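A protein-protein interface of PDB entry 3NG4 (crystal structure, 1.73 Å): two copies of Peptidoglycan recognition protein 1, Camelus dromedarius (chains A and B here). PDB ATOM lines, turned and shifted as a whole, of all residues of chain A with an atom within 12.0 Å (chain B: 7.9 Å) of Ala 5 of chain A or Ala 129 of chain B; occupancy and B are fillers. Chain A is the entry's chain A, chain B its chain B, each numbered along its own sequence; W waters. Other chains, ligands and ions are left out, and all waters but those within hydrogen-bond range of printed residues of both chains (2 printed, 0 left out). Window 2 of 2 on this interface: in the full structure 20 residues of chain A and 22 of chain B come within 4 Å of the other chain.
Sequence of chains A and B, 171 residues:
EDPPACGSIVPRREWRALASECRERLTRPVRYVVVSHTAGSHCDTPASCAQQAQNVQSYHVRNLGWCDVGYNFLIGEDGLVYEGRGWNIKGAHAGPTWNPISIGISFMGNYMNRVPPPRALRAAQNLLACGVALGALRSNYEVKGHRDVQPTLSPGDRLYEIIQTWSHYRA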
ATOM      1  N   GLU A   1     -10.838 -15.452  21.387  1.00  0.00           N
ATOM      2  CA  GLU A   1     -11.715 -14.297  21.799  1.00  0.00           C
ATOM      3  C   GLU A   1     -11.461 -13.064  20.879  1.00  0.00           C
ATOM      4  O   GLU A   1     -12.381 -12.602  20.138  1.00  0.00           O
ATOM      5  CB  GLU A   1     -11.495 -13.959  23.298  1.00  0.00           C
ATOM      6  CG  GLU A   1     -12.329 -12.799  23.850  1.00  0.00           C
ATOM      7  CD  GLU A   1     -13.815 -13.122  23.961  1.00  0.00           C
ATOM      8  OE1 GLU A   1     -14.324 -13.163  25.099  1.00  0.00           O
ATOM      9  OE2 GLU A   1     -14.477 -13.335  22.916  1.00  0.00           O
ATOM     10  N   ASP A   2     -10.217 -12.551  20.966  1.00  0.00           N
ATOM     11  CA  ASP A   2      -9.659 -11.441  20.140  1.00  0.00           C
ATOM     12  C   ASP A   2      -8.303 -11.999  19.610  1.00  0.00           C
ATOM     13  O   ASP A   2      -7.471 -12.501  20.451  1.00  0.00           O
ATOM     14  CB  ASP A   2      -9.388 -10.164  20.996  1.00  0.00           C
ATOM     15  CG  ASP A   2     -10.528  -9.851  22.009  1.00  0.00           C
ATOM     16  OD1 ASP A   2     -11.364  -8.959  21.708  1.00  0.00           O
ATOM     17  OD2 ASP A   2     -10.586 -10.498  23.102  1.00  0.00           O
ATOM     18  N   PRO A   3      -8.056 -11.941  18.246  1.00  0.00           N
ATOM     19  CA  PRO A   3      -6.786 -12.606  17.751  1.00  0.00           C
ATOM     20  C   PRO A   3      -5.348 -11.908  17.786  1.00  0.00           C
ATOM     21  O   PRO A   3      -4.397 -12.442  17.160  1.00  0.00           O
ATOM     22  CB  PRO A   3      -7.165 -13.084  16.312  1.00  0.00           C
ATOM     23  CG  PRO A   3      -8.751 -12.948  16.250  1.00  0.00           C
ATOM     24  CD  PRO A   3      -9.075 -11.769  17.134  1.00  0.00           C
ATOM     25  N   PRO A   4      -5.156 -10.778  18.558  1.00  0.00           N
ATOM     26  CA  PRO A   4      -3.955  -9.944  18.306  1.00  0.00           C
ATOM     27  C   PRO A   4      -2.607 -10.556  18.781  1.00  0.00           C
ATOM     28  O   PRO A   4      -2.487 -11.083  19.921  1.00  0.00           O
ATOM     29  CB  PRO A   4      -4.261  -8.635  19.068  1.00  0.00           C
ATOM     30  CG  PRO A   4      -5.071  -9.112  20.285  1.00  0.00           C
ATOM     31  CD  PRO A   4      -5.844 -10.345  19.809  1.00  0.00           C
ATOM     32  N   ALA A   5      -1.618 -10.484  17.871  1.00  0.00           N
ATOM     33  CA  ALA A   5      -0.230 -10.798  18.209  1.00  0.00           C
ATOM     34  C   ALA A   5       0.214  -9.820  19.317  1.00  0.00           C
ATOM     35  O   ALA A   5      -0.303  -8.681  19.388  1.00  0.00           O
ATOM     36  CB  ALA A   5       0.670 -10.639  16.951  1.00  0.00           C
ATOM     37  N   CYS A   6       1.159 -10.248  20.164  1.00  0.00           N
ATOM     38  CA  CYS A   6       1.565  -9.454  21.329  1.00  0.00           C
ATOM     39  C   CYS A   6       2.783 -10.040  22.025  1.00  0.00           C
ATOM     40  O   CYS A   6       2.811 -11.211  22.437  1.00  0.00           O
ATOM     41  CB  CYS A   6       0.427  -9.363  22.362  1.00  0.00           C
ATOM     42  SG  CYS A   6       0.712  -8.088  23.621  1.00  0.00           S
ATOM     43  N   GLY A   7       3.797  -9.229  22.163  1.00  0.00           N
ATOM     44  CA  GLY A   7       4.983  -9.691  22.798  1.00  0.00           C
ATOM     45  C   GLY A   7       5.733 -10.582  21.860  1.00  0.00           C
ATOM     46  O   GLY A   7       5.407 -10.686  20.695  1.00  0.00           O
ATOM     47  N   SER A   8       6.762 -11.200  22.397  1.00  0.00           N
ATOM     48  CA  SER A   8       7.607 -12.072  21.666  1.00  0.00           C
ATOM     49  C   SER A   8       7.890 -13.099  22.681  1.00  0.00           C
ATOM     50  O   SER A   8       8.412 -12.796  23.706  1.00  0.00           O
ATOM     51  CB  SER A   8       8.943 -11.417  21.340  1.00  0.00           C
ATOM     52  OG  SER A   8       8.916 -10.731  20.135  1.00  0.00           O
ATOM     53  N   ILE A   9       7.559 -14.316  22.386  1.00  0.00           N
ATOM     54  CA  ILE A   9       7.860 -15.350  23.317  1.00  0.00           C
ATOM     55  C   ILE A   9       8.687 -16.452  22.692  1.00  0.00           C
ATOM     56  O   ILE A   9       8.444 -16.826  21.619  1.00  0.00           O
ATOM     57  CB  ILE A   9       6.614 -15.888  23.871  1.00  0.00           C
ATOM     58  CG1 ILE A   9       6.081 -14.886  24.854  1.00  0.00           C
ATOM     59  CG2 ILE A   9       6.907 -17.096  24.574  1.00  0.00           C
ATOM     60  CD1 ILE A   9       4.850 -15.174  25.359  1.00  0.00           C
ATOM     61  N   TRP A  87      -0.222 -19.415  29.392  1.00  0.00           N
ATOM     62  CA  TRP A  87      -1.295 -18.659  30.011  1.00  0.00           C
ATOM     63  C   TRP A  87      -2.435 -19.545  30.536  1.00  0.00           C
ATOM     64  O   TRP A  87      -3.150 -19.138  31.400  1.00  0.00           O
ATOM     65  CB  TRP A  87      -1.922 -17.707  29.013  1.00  0.00           C
ATOM     66  CG  TRP A  87      -1.034 -16.566  28.607  1.00  0.00           C
ATOM     67  CD1 TRP A  87      -0.585 -16.293  27.344  1.00  0.00           C
ATOM     68  CD2 TRP A  87      -0.563 -15.527  29.434  1.00  0.00           C
ATOM     69  NE1 TRP A  87       0.202 -15.159  27.353  1.00  0.00           N
ATOM     70  CE2 TRP A  87       0.229 -14.664  28.619  1.00  0.00           C
ATOM     71  CE3 TRP A  87      -0.668 -15.245  30.805  1.00  0.00           C
ATOM     72  CZ2 TRP A  87       0.862 -13.561  29.131  1.00  0.00           C
ATOM     73  CZ3 TRP A  87      -0.013 -14.136  31.292  1.00  0.00           C
ATOM     74  CH2 TRP A  87       0.744 -13.322  30.475  1.00  0.00           C
ATOM     75  N   ASN A 126       5.998  -6.299  29.733  1.00  0.00           N
ATOM     76  CA  ASN A 126       5.336  -6.400  28.408  1.00  0.00           C
ATOM     77  C   ASN A 126       4.570  -7.688  28.287  1.00  0.00           C
ATOM     78  O   ASN A 126       3.553  -7.769  27.640  1.00  0.00           O
ATOM     79  CB  ASN A 126       6.339  -6.268  27.292  1.00  0.00           C
ATOM     80  CG  ASN A 126       6.739  -4.806  27.027  1.00  0.00           C
ATOM     81  OD1 ASN A 126       6.357  -3.855  27.759  1.00  0.00           O
ATOM     82  ND2 ASN A 126       7.451  -4.613  25.947  1.00  0.00           N
ATOM     83  N   LEU A 127       5.105  -8.749  28.885  1.00  0.00           N
ATOM     84  CA  LEU A 127       4.445 -10.038  28.803  1.00  0.00           C
ATOM     85  C   LEU A 127       3.088  -9.919  29.533  1.00  0.00           C
ATOM     86  O   LEU A 127       2.108 -10.409  29.022  1.00  0.00           O
ATOM     87  CB  LEU A 127       5.300 -11.143  29.467  1.00  0.00           C
ATOM     88  CG  LEU A 127       4.548 -12.390  29.847  1.00  0.00           C
ATOM     89  CD1 LEU A 127       4.191 -13.246  28.592  1.00  0.00           C
ATOM     90  CD2 LEU A 127       5.384 -13.226  30.809  1.00  0.00           C
ATOM     91  N   LEU A 128       3.093  -9.255  30.658  1.00  0.00           N
ATOM     92  CA  LEU A 128       1.867  -9.104  31.467  1.00  0.00           C
ATOM     93  C   LEU A 128       0.859  -8.275  30.676  1.00  0.00           C
ATOM     94  O   LEU A 128      -0.279  -8.636  30.597  1.00  0.00           O
ATOM     95  CB  LEU A 128       2.189  -8.462  32.790  1.00  0.00           C
ATOM     96  CG  LEU A 128       3.198  -9.305  33.619  1.00  0.00           C
ATOM     97  CD1 LEU A 128       3.274  -8.717  35.014  1.00  0.00           C
ATOM     98  CD2 LEU A 128       2.774 -10.783  33.672  1.00  0.00           C
ATOM     99  N   ALA A 129       1.317  -7.196  30.052  1.00  0.00           N
ATOM    100  CA  ALA A 129       0.411  -6.414  29.195  1.00  0.00           C
ATOM    101  C   ALA A 129      -0.233  -7.291  28.152  1.00  0.00           C
ATOM    102  O   ALA A 129      -1.398  -7.116  27.861  1.00  0.00           O
ATOM    103  CB  ALA A 129       1.148  -5.242  28.566  1.00  0.00           C
ATOM    104  N   CYS A 130       0.544  -8.220  27.567  1.00  0.00           N
ATOM    105  CA  CYS A 130       0.035  -9.119  26.550  1.00  0.00           C
ATOM    106  C   CYS A 130      -0.978 -10.059  27.131  1.00  0.00           C
ATOM    107  O   CYS A 130      -1.972 -10.420  26.481  1.00  0.00           O
ATOM    108  CB  CYS A 130       1.145  -9.930  25.877  1.00  0.00           C
ATOM    109  SG  CYS A 130       2.135  -8.865  24.820  1.00  0.00           S
ATOM    110  N   GLY A 131      -0.712 -10.499  28.349  1.00  0.00           N
ATOM    111  CA  GLY A 131      -1.659 -11.384  28.999  1.00  0.00           C
ATOM    112  C   GLY A 131      -3.006 -10.723  29.137  1.00  0.00           C
ATOM    113  O   GLY A 131      -4.024 -11.386  28.930  1.00  0.00           O
ATOM    114  N   VAL A 132      -3.020  -9.450  29.501  1.00  0.00           N
ATOM    115  CA  VAL A 132      -4.280  -8.709  29.597  1.00  0.00           C
ATOM    116  C   VAL A 132      -5.028  -8.650  28.211  1.00  0.00           C
ATOM    117  O   VAL A 132      -6.207  -8.933  28.105  1.00  0.00           O
ATOM    118  CB  VAL A 132      -4.051  -7.322  30.118  1.00  0.00           C
ATOM    119  CG1 VAL A 132      -5.365  -6.488  30.119  1.00  0.00           C
ATOM    120  CG2 VAL A 132      -3.455  -7.361  31.601  1.00  0.00           C
ATOM    121  N   ALA A 133      -4.301  -8.321  27.157  1.00  0.00           N
ATOM    122  CA  ALA A 133      -4.950  -8.178  25.858  1.00  0.00           C
ATOM    123  C   ALA A 133      -5.496  -9.523  25.368  1.00  0.00           C
ATOM    124  O   ALA A 133      -6.491  -9.578  24.626  1.00  0.00           O
ATOM    125  CB  ALA A 133      -3.954  -7.615  24.840  1.00  0.00           C
ATOM    126  N   LEU A 134      -4.881 -10.615  25.764  1.00  0.00           N
ATOM    127  CA  LEU A 134      -5.335 -11.919  25.395  1.00  0.00           C
ATOM    128  C   LEU A 134      -6.523 -12.369  26.210  1.00  0.00           C
ATOM    129  O   LEU A 134      -7.147 -13.330  25.870  1.00  0.00           O
ATOM    130  CB  LEU A 134      -4.235 -12.935  25.571  1.00  0.00           C
ATOM    131  CG  LEU A 134      -3.157 -12.963  24.458  1.00  0.00           C
ATOM    132  CD1 LEU A 134      -2.113 -13.957  24.844  1.00  0.00           C
ATOM    133  CD2 LEU A 134      -3.811 -13.379  23.160  1.00  0.00           C
ATOM    134  N   GLY A 135      -6.776 -11.677  27.312  1.00  0.00           N
ATOM    135  CA  GLY A 135      -7.828 -12.090  28.253  1.00  0.00           C
ATOM    136  C   GLY A 135      -7.371 -13.183  29.195  1.00  0.00           C
ATOM    137  O   GLY A 135      -8.172 -13.750  29.960  1.00  0.00           O
ATOM    138  N   CYS B   6       5.443  -0.641  25.106  1.00  0.00           N
ATOM    139  CA  CYS B   6       5.312  -1.971  24.505  1.00  0.00           C
ATOM    140  C   CYS B   6       6.419  -2.293  23.496  1.00  0.00           C
ATOM    141  O   CYS B   6       7.154  -1.404  23.061  1.00  0.00           O
ATOM    142  CB  CYS B   6       3.930  -2.144  23.861  1.00  0.00           C
ATOM    143  SG  CYS B   6       3.376  -0.929  22.616  1.00  0.00           S
ATOM    144  N   GLY B   7       6.532  -3.571  23.140  1.00  0.00           N
ATOM    145  CA  GLY B   7       7.494  -4.019  22.135  1.00  0.00           C
ATOM    146  C   GLY B   7       8.848  -4.450  22.670  1.00  0.00           C
ATOM    147  O   GLY B   7       9.678  -4.960  21.913  1.00  0.00           O
ATOM    148  N   TRP B  87       8.701   5.998  17.067  1.00  0.00           N
ATOM    149  CA  TRP B  87       7.403   6.063  16.450  1.00  0.00           C
ATOM    150  C   TRP B  87       6.986   7.423  15.870  1.00  0.00           C
ATOM    151  O   TRP B  87       6.118   7.473  14.978  1.00  0.00           O
ATOM    152  CB  TRP B  87       6.336   5.665  17.512  1.00  0.00           C
ATOM    153  CG  TRP B  87       6.429   4.196  17.867  1.00  0.00           C
ATOM    154  CD1 TRP B  87       6.664   3.680  19.088  1.00  0.00           C
ATOM    155  CD2 TRP B  87       6.163   3.101  17.002  1.00  0.00           C
ATOM    156  NE1 TRP B  87       6.639   2.301  19.031  1.00  0.00           N
ATOM    157  CE2 TRP B  87       6.365   1.924  17.747  1.00  0.00           C
ATOM    158  CE3 TRP B  87       5.866   2.990  15.636  1.00  0.00           C
ATOM    159  CZ2 TRP B  87       6.174   0.656  17.201  1.00  0.00           C
ATOM    160  CZ3 TRP B  87       5.724   1.720  15.088  1.00  0.00           C
ATOM    161  CH2 TRP B  87       5.867   0.580  15.867  1.00  0.00           C
ATOM    162  N   ARG B 122      10.022 -12.529  15.263  1.00  0.00           N
ATOM    163  CA  ARG B 122       9.042 -12.297  16.301  1.00  0.00           C
ATOM    164  C   ARG B 122       9.163 -10.901  16.867  1.00  0.00           C
ATOM    165  O   ARG B 122       8.222 -10.294  17.192  1.00  0.00           O
ATOM    166  CB  ARG B 122       9.231 -13.254  17.471  1.00  0.00           C
ATOM    167  CG  ARG B 122       9.027 -14.670  17.181  1.00  0.00           C
ATOM    168  CD  ARG B 122       8.741 -15.360  18.426  1.00  0.00           C
ATOM    169  NE  ARG B 122       9.930 -15.548  19.195  1.00  0.00           N
ATOM    170  CZ  ARG B 122      10.803 -16.505  18.995  1.00  0.00           C
ATOM    171  NH1 ARG B 122      11.848 -16.593  19.745  1.00  0.00           N
ATOM    172  NH2 ARG B 122      10.618 -17.388  18.057  1.00  0.00           N
ATOM    173  N   ALA B 123      10.392 -10.444  17.009  1.00  0.00           N
ATOM    174  CA  ALA B 123      10.619  -9.148  17.582  1.00  0.00           C
ATOM    175  C   ALA B 123       9.964  -8.105  16.715  1.00  0.00           C
ATOM    176  O   ALA B 123       9.368  -7.171  17.186  1.00  0.00           O
ATOM    177  CB  ALA B 123      12.114  -8.869  17.778  1.00  0.00           C
ATOM    178  N   ALA B 124      10.091  -8.299  15.433  1.00  0.00           N
ATOM    179  CA  ALA B 124       9.500  -7.350  14.505  1.00  0.00           C
ATOM    180  C   ALA B 124       7.976  -7.329  14.602  1.00  0.00           C
ATOM    181  O   ALA B 124       7.399  -6.327  14.638  1.00  0.00           O
ATOM    182  CB  ALA B 124       9.951  -7.632  13.121  1.00  0.00           C
ATOM    183  N   GLN B 125       7.355  -8.476  14.677  1.00  0.00           N
ATOM    184  CA  GLN B 125       5.916  -8.524  14.816  1.00  0.00           C
ATOM    185  C   GLN B 125       5.480  -7.949  16.136  1.00  0.00           C
ATOM    186  O   GLN B 125       4.567  -7.213  16.182  1.00  0.00           O
ATOM    187  CB  GLN B 125       5.427  -9.936  14.625  1.00  0.00           C
ATOM    188  CG  GLN B 125       5.977 -10.506  13.422  1.00  0.00           C
ATOM    189  CD  GLN B 125       5.244 -10.077  12.227  1.00  0.00           C
ATOM    190  OE1 GLN B 125       4.476  -9.169  12.255  1.00  0.00           O
ATOM    191  NE2 GLN B 125       5.407 -10.795  11.204  1.00  0.00           N
ATOM    192  N   ASN B 126       6.191  -8.271  17.203  1.00  0.00           N
ATOM    193  CA  ASN B 126       5.930  -7.673  18.530  1.00  0.00           C
ATOM    194  C   ASN B 126       5.889  -6.133  18.364  1.00  0.00           C
ATOM    195  O   ASN B 126       4.986  -5.442  18.867  1.00  0.00           O
ATOM    196  CB  ASN B 126       7.056  -8.107  19.502  1.00  0.00           C
ATOM    197  CG  ASN B 126       6.989  -7.424  20.944  1.00  0.00           C
ATOM    198  OD1 ASN B 126       6.128  -6.598  21.236  1.00  0.00           O
ATOM    199  ND2 ASN B 126       7.930  -7.781  21.810  1.00  0.00           N
ATOM    200  N   LEU B 127       6.888  -5.598  17.674  1.00  0.00           N
ATOM    201  CA  LEU B 127       7.018  -4.180  17.497  1.00  0.00           C
ATOM    202  C   LEU B 127       5.835  -3.543  16.775  1.00  0.00           C
ATOM    203  O   LEU B 127       5.262  -2.550  17.237  1.00  0.00           O
ATOM    204  CB  LEU B 127       8.309  -3.832  16.761  1.00  0.00           C
ATOM    205  CG  LEU B 127       8.512  -2.392  16.432  1.00  0.00           C
ATOM    206  CD1 LEU B 127       8.889  -1.569  17.716  1.00  0.00           C
ATOM    207  CD2 LEU B 127       9.665  -2.291  15.419  1.00  0.00           C
ATOM    208  N   LEU B 128       5.459  -4.135  15.680  1.00  0.00           N
ATOM    209  CA  LEU B 128       4.365  -3.617  14.874  1.00  0.00           C
ATOM    210  C   LEU B 128       3.025  -3.711  15.586  1.00  0.00           C
ATOM    211  O   LEU B 128       2.265  -2.776  15.561  1.00  0.00           O
ATOM    212  CB  LEU B 128       4.332  -4.349  13.520  1.00  0.00           C
ATOM    213  CG  LEU B 128       5.670  -4.174  12.775  1.00  0.00           C
ATOM    214  CD1 LEU B 128       5.529  -4.694  11.345  1.00  0.00           C
ATOM    215  CD2 LEU B 128       6.123  -2.754  12.703  1.00  0.00           C
ATOM    216  N   ALA B 129       2.818  -4.807  16.329  1.00  0.00           N
ATOM    217  CA  ALA B 129       1.562  -4.983  17.105  1.00  0.00           C
ATOM    218  C   ALA B 129       1.532  -3.819  18.106  1.00  0.00           C
ATOM    219  O   ALA B 129       0.471  -3.176  18.336  1.00  0.00           O
ATOM    220  CB  ALA B 129       1.615  -6.320  17.857  1.00  0.00           C
ATOM    221  N   CYS B 130       2.686  -3.552  18.735  1.00  0.00           N
ATOM    222  CA  CYS B 130       2.842  -2.489  19.676  1.00  0.00           C
ATOM    223  C   CYS B 130       2.554  -1.132  19.040  1.00  0.00           C
ATOM    224  O   CYS B 130       1.909  -0.270  19.650  1.00  0.00           O
ATOM    225  CB  CYS B 130       4.263  -2.523  20.279  1.00  0.00           C
ATOM    226  SG  CYS B 130       4.575  -0.929  21.011  1.00  0.00           S
ATOM    227  N   GLY B 131       2.962  -0.944  17.804  1.00  0.00           N
ATOM    228  CA  GLY B 131       2.712   0.330  17.164  1.00  0.00           C
ATOM    229  C   GLY B 131       1.221   0.528  16.973  1.00  0.00           C
ATOM    230  O   GLY B 131       0.710   1.646  17.079  1.00  0.00           O
ATOM    231  N   VAL B 132       0.528  -0.552  16.665  1.00  0.00           N
ATOM    232  CA  VAL B 132      -0.937  -0.420  16.443  1.00  0.00           C
ATOM    233  C   VAL B 132      -1.546  -0.079  17.818  1.00  0.00           C
ATOM    234  O   VAL B 132      -2.351   0.861  17.957  1.00  0.00           O
ATOM    235  CB  VAL B 132      -1.521  -1.731  15.888  1.00  0.00           C
ATOM    236  CG1 VAL B 132      -3.042  -1.711  16.048  1.00  0.00           C
ATOM    237  CG2 VAL B 132      -1.109  -1.857  14.392  1.00  0.00           C
ATOM    238  N   ALA B 133      -1.122  -0.801  18.851  1.00  0.00           N
ATOM    239  CA  ALA B 133      -1.722  -0.610  20.208  1.00  0.00           C
ATOM    240  C   ALA B 133      -1.519   0.826  20.644  1.00  0.00           C
ATOM    241  O   ALA B 133      -2.337   1.373  21.392  1.00  0.00           O
ATOM    242  CB  ALA B 133      -1.060  -1.546  21.227  1.00  0.00           C
ATOM    243  N   LEU B 134      -0.417   1.449  20.223  1.00  0.00           N
ATOM    244  CA  LEU B 134      -0.112   2.856  20.570  1.00  0.00           C
ATOM    245  C   LEU B 134      -0.831   3.853  19.726  1.00  0.00           C
ATOM    246  O   LEU B 134      -0.925   5.030  20.078  1.00  0.00           O
ATOM    247  CB  LEU B 134       1.396   3.148  20.431  1.00  0.00           C
ATOM    248  CG  LEU B 134       2.360   2.508  21.426  1.00  0.00           C
ATOM    249  CD1 LEU B 134       3.773   2.843  20.994  1.00  0.00           C
ATOM    250  CD2 LEU B 134       2.024   2.973  22.923  1.00  0.00           C
ATOM    251  N   GLY B 135      -1.310   3.435  18.563  1.00  0.00           N
ATOM    252  CA  GLY B 135      -1.941   4.415  17.691  1.00  0.00           C
ATOM    253  C   GLY B 135      -0.929   4.987  16.731  1.00  0.00           C
ATOM    254  O   GLY B 135      -1.241   5.877  15.927  1.00  0.00           O
ATOM    255  N   ALA B 136       0.316   4.470  16.823  1.00  0.00           N
ATOM    256  CA  ALA B 136       1.408   4.999  15.972  1.00  0.00           C
ATOM    257  C   ALA B 136       1.216   4.469  14.551  1.00  0.00           C
ATOM    258  O   ALA B 136       1.489   5.191  13.574  1.00  0.00           O
ATOM    259  CB  ALA B 136       2.795   4.526  16.514  1.00  0.00           C
ATOM    260  N   LEU B 137       0.711   3.234  14.436  1.00  0.00           N
ATOM    261  CA  LEU B 137       0.447   2.648  13.168  1.00  0.00           C
ATOM    262  C   LEU B 137      -1.078   2.396  13.068  1.00  0.00           C
ATOM    263  O   LEU B 137      -1.700   2.000  14.066  1.00  0.00           O
ATOM    264  CB  LEU B 137       1.117   1.322  13.043  1.00  0.00           C
ATOM    265  CG  LEU B 137       2.646   1.151  12.951  1.00  0.00           C
ATOM    266  CD1 LEU B 137       2.969  -0.330  12.964  1.00  0.00           C
ATOM    267  CD2 LEU B 137       3.257   1.809  11.723  1.00  0.00           C
ATOM    268  N   TYR B 141      -2.226  -1.556   8.942  1.00  0.00           N
ATOM    269  CA  TYR B 141      -1.033  -1.041   8.304  1.00  0.00           C
ATOM    270  C   TYR B 141      -0.557  -1.963   7.215  1.00  0.00           C
ATOM    271  O   TYR B 141      -0.901  -3.148   7.170  1.00  0.00           O
ATOM    272  CB  TYR B 141       0.072  -0.838   9.361  1.00  0.00           C
ATOM    273  CG  TYR B 141       0.514  -2.107  10.009  1.00  0.00           C
ATOM    274  CD1 TYR B 141       1.537  -2.876   9.440  1.00  0.00           C
ATOM    275  CD2 TYR B 141      -0.086  -2.560  11.200  1.00  0.00           C
ATOM    276  CE1 TYR B 141       1.957  -4.071  10.065  1.00  0.00           C
ATOM    277  CE2 TYR B 141       0.321  -3.778  11.824  1.00  0.00           C
ATOM    278  CZ  TYR B 141       1.368  -4.493  11.258  1.00  0.00           C
ATOM    279  OH  TYR B 141       1.755  -5.680  11.826  1.00  0.00           O
ATOM    280  N   HIS B 168       0.127  -8.626   6.786  1.00  0.00           N
ATOM    281  CA  HIS B 168       0.020  -7.186   6.511  1.00  0.00           C
ATOM    282  C   HIS B 168       0.827  -6.746   5.275  1.00  0.00           C
ATOM    283  O   HIS B 168       0.783  -5.559   4.953  1.00  0.00           O
ATOM    284  CB  HIS B 168       0.471  -6.348   7.706  1.00  0.00           C
ATOM    285  CG  HIS B 168      -0.572  -6.223   8.785  1.00  0.00           C
ATOM    286  ND1 HIS B 168      -0.820  -7.228   9.716  1.00  0.00           N
ATOM    287  CD2 HIS B 168      -1.414  -5.223   9.067  1.00  0.00           C
ATOM    288  CE1 HIS B 168      -1.795  -6.824  10.535  1.00  0.00           C
ATOM    289  NE2 HIS B 168      -2.176  -5.612  10.150  1.00  0.00           N
HETATM  290  O   HOH W   1       7.020  -7.250  24.464  1.00  0.00           O
HETATM  291  O   HOH W   2       3.506  -6.223  21.169  1.00  0.00           O
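Of the 21 printed residues of chain B, 6 touch a printed residue of chain A.
The backbone NH of Ala 123 of chain B sits close to the side-chain hydroxyl of Ser 8 of chain A (3.5 Å). The backbone carbonyl oxygen (O) of Ile 9 of chain A sits at hydrogen-bond distance from the guanidinium group (NE) of Arg 122 of chain B, at 3.1 Å. The backbone carbonyl oxygen (O) of Arg 122 of chain B is in hydrogen-bond range of the side-chain hydroxyl (OG) of Ser 8 of chain A, at 3.1 Å. The side-chain amide nitrogen (ND2) of Asn 126 of chain A lies close to the backbone NH (N) of Gly 7 of chain B (3.1 Å).
O of Ala 5 of chain A touches CB of Ala 129 of chain B, 3.4 Å away. Gly 7 of chain A touches Asn 126 of chain B. OG of Ser 8 of chain A touches CB of Asn 126 of chain B (3.3 Å). ND2 of Asn 126 of chain A touches C of Cys 6 of chain B (3.5 Å).
Of chain B, only Ala 129 (3.4 Å) comes within 4 Å of Ala 5 of chain A. No residue of chain A comes within 4 Å of Leu 127 of chain B. No residue of chain A comes within 4 Å of Leu 128 of chain B. No residue of chain A comes within 4 Å of Gly 131 of chain B. No residue of chain A comes within 4 Å of Ala 133 of chain B. Of the printed residues of chain B, Ile 9 of chain A touches Arg 122. Of the printed residues of chain B, Asn 126 of chain A touches Cys 6 (3.5 Å) and Gly 7 (3.1 Å). The nearest residue of chain B that does not touch Ala 5 of chain A is Gln 125 of chain B (5.2 Å). The nearest residue of chain A that does not touch Ala 129 of chain B is Cys 6 of chain A (4.6 Å).
Gly 7 of chain A touches Asn 126 of chain B, and with the chains exchanged Asn 126 of chain A touches Gly 7 of chain B. Asn 126 of chain A touches Cys 6 of chain B, but with the chains exchanged Cys 6 of chain A does not touch Asn 126 of chain B (4.9 Å). Positions printed for both chains: 6, 7, 87, 126, 127, 128, 129, 130, 131, 132, 133, 134 and 135.
The backbone carbonyl oxygen (O) of Gly 7 of chain B is in hydrogen-bond range of the side-chain amide nitrogen (ND2) of Asn 126 of chain B (3.3 Å). SG of Cys 130 of chain B forms a disulfide with SG of Cys 6 of chain B. SG of Cys 130 of chain A is in hydrogen-bond range of N of Gly 7 of chain A (3.2 Å). The side-chain sulfur (SG) of Cys 6 of chain A is disulfide-bonded to the side-chain sulfur (SG) of Cys 130 of chain A, at 2.0 Å.
Water W2 lies within hydrogen-bond range of OD1 of Asn 126 of chain B and N of Gly 7 of chain A. Water W1 lies within hydrogen-bond range of the side-chain amide nitrogen (ND2) of Asn 126 of chain B (2.9 Å) and the side-chain amide nitrogen (ND2) of Asn 126 of chain A (3.1 Å).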
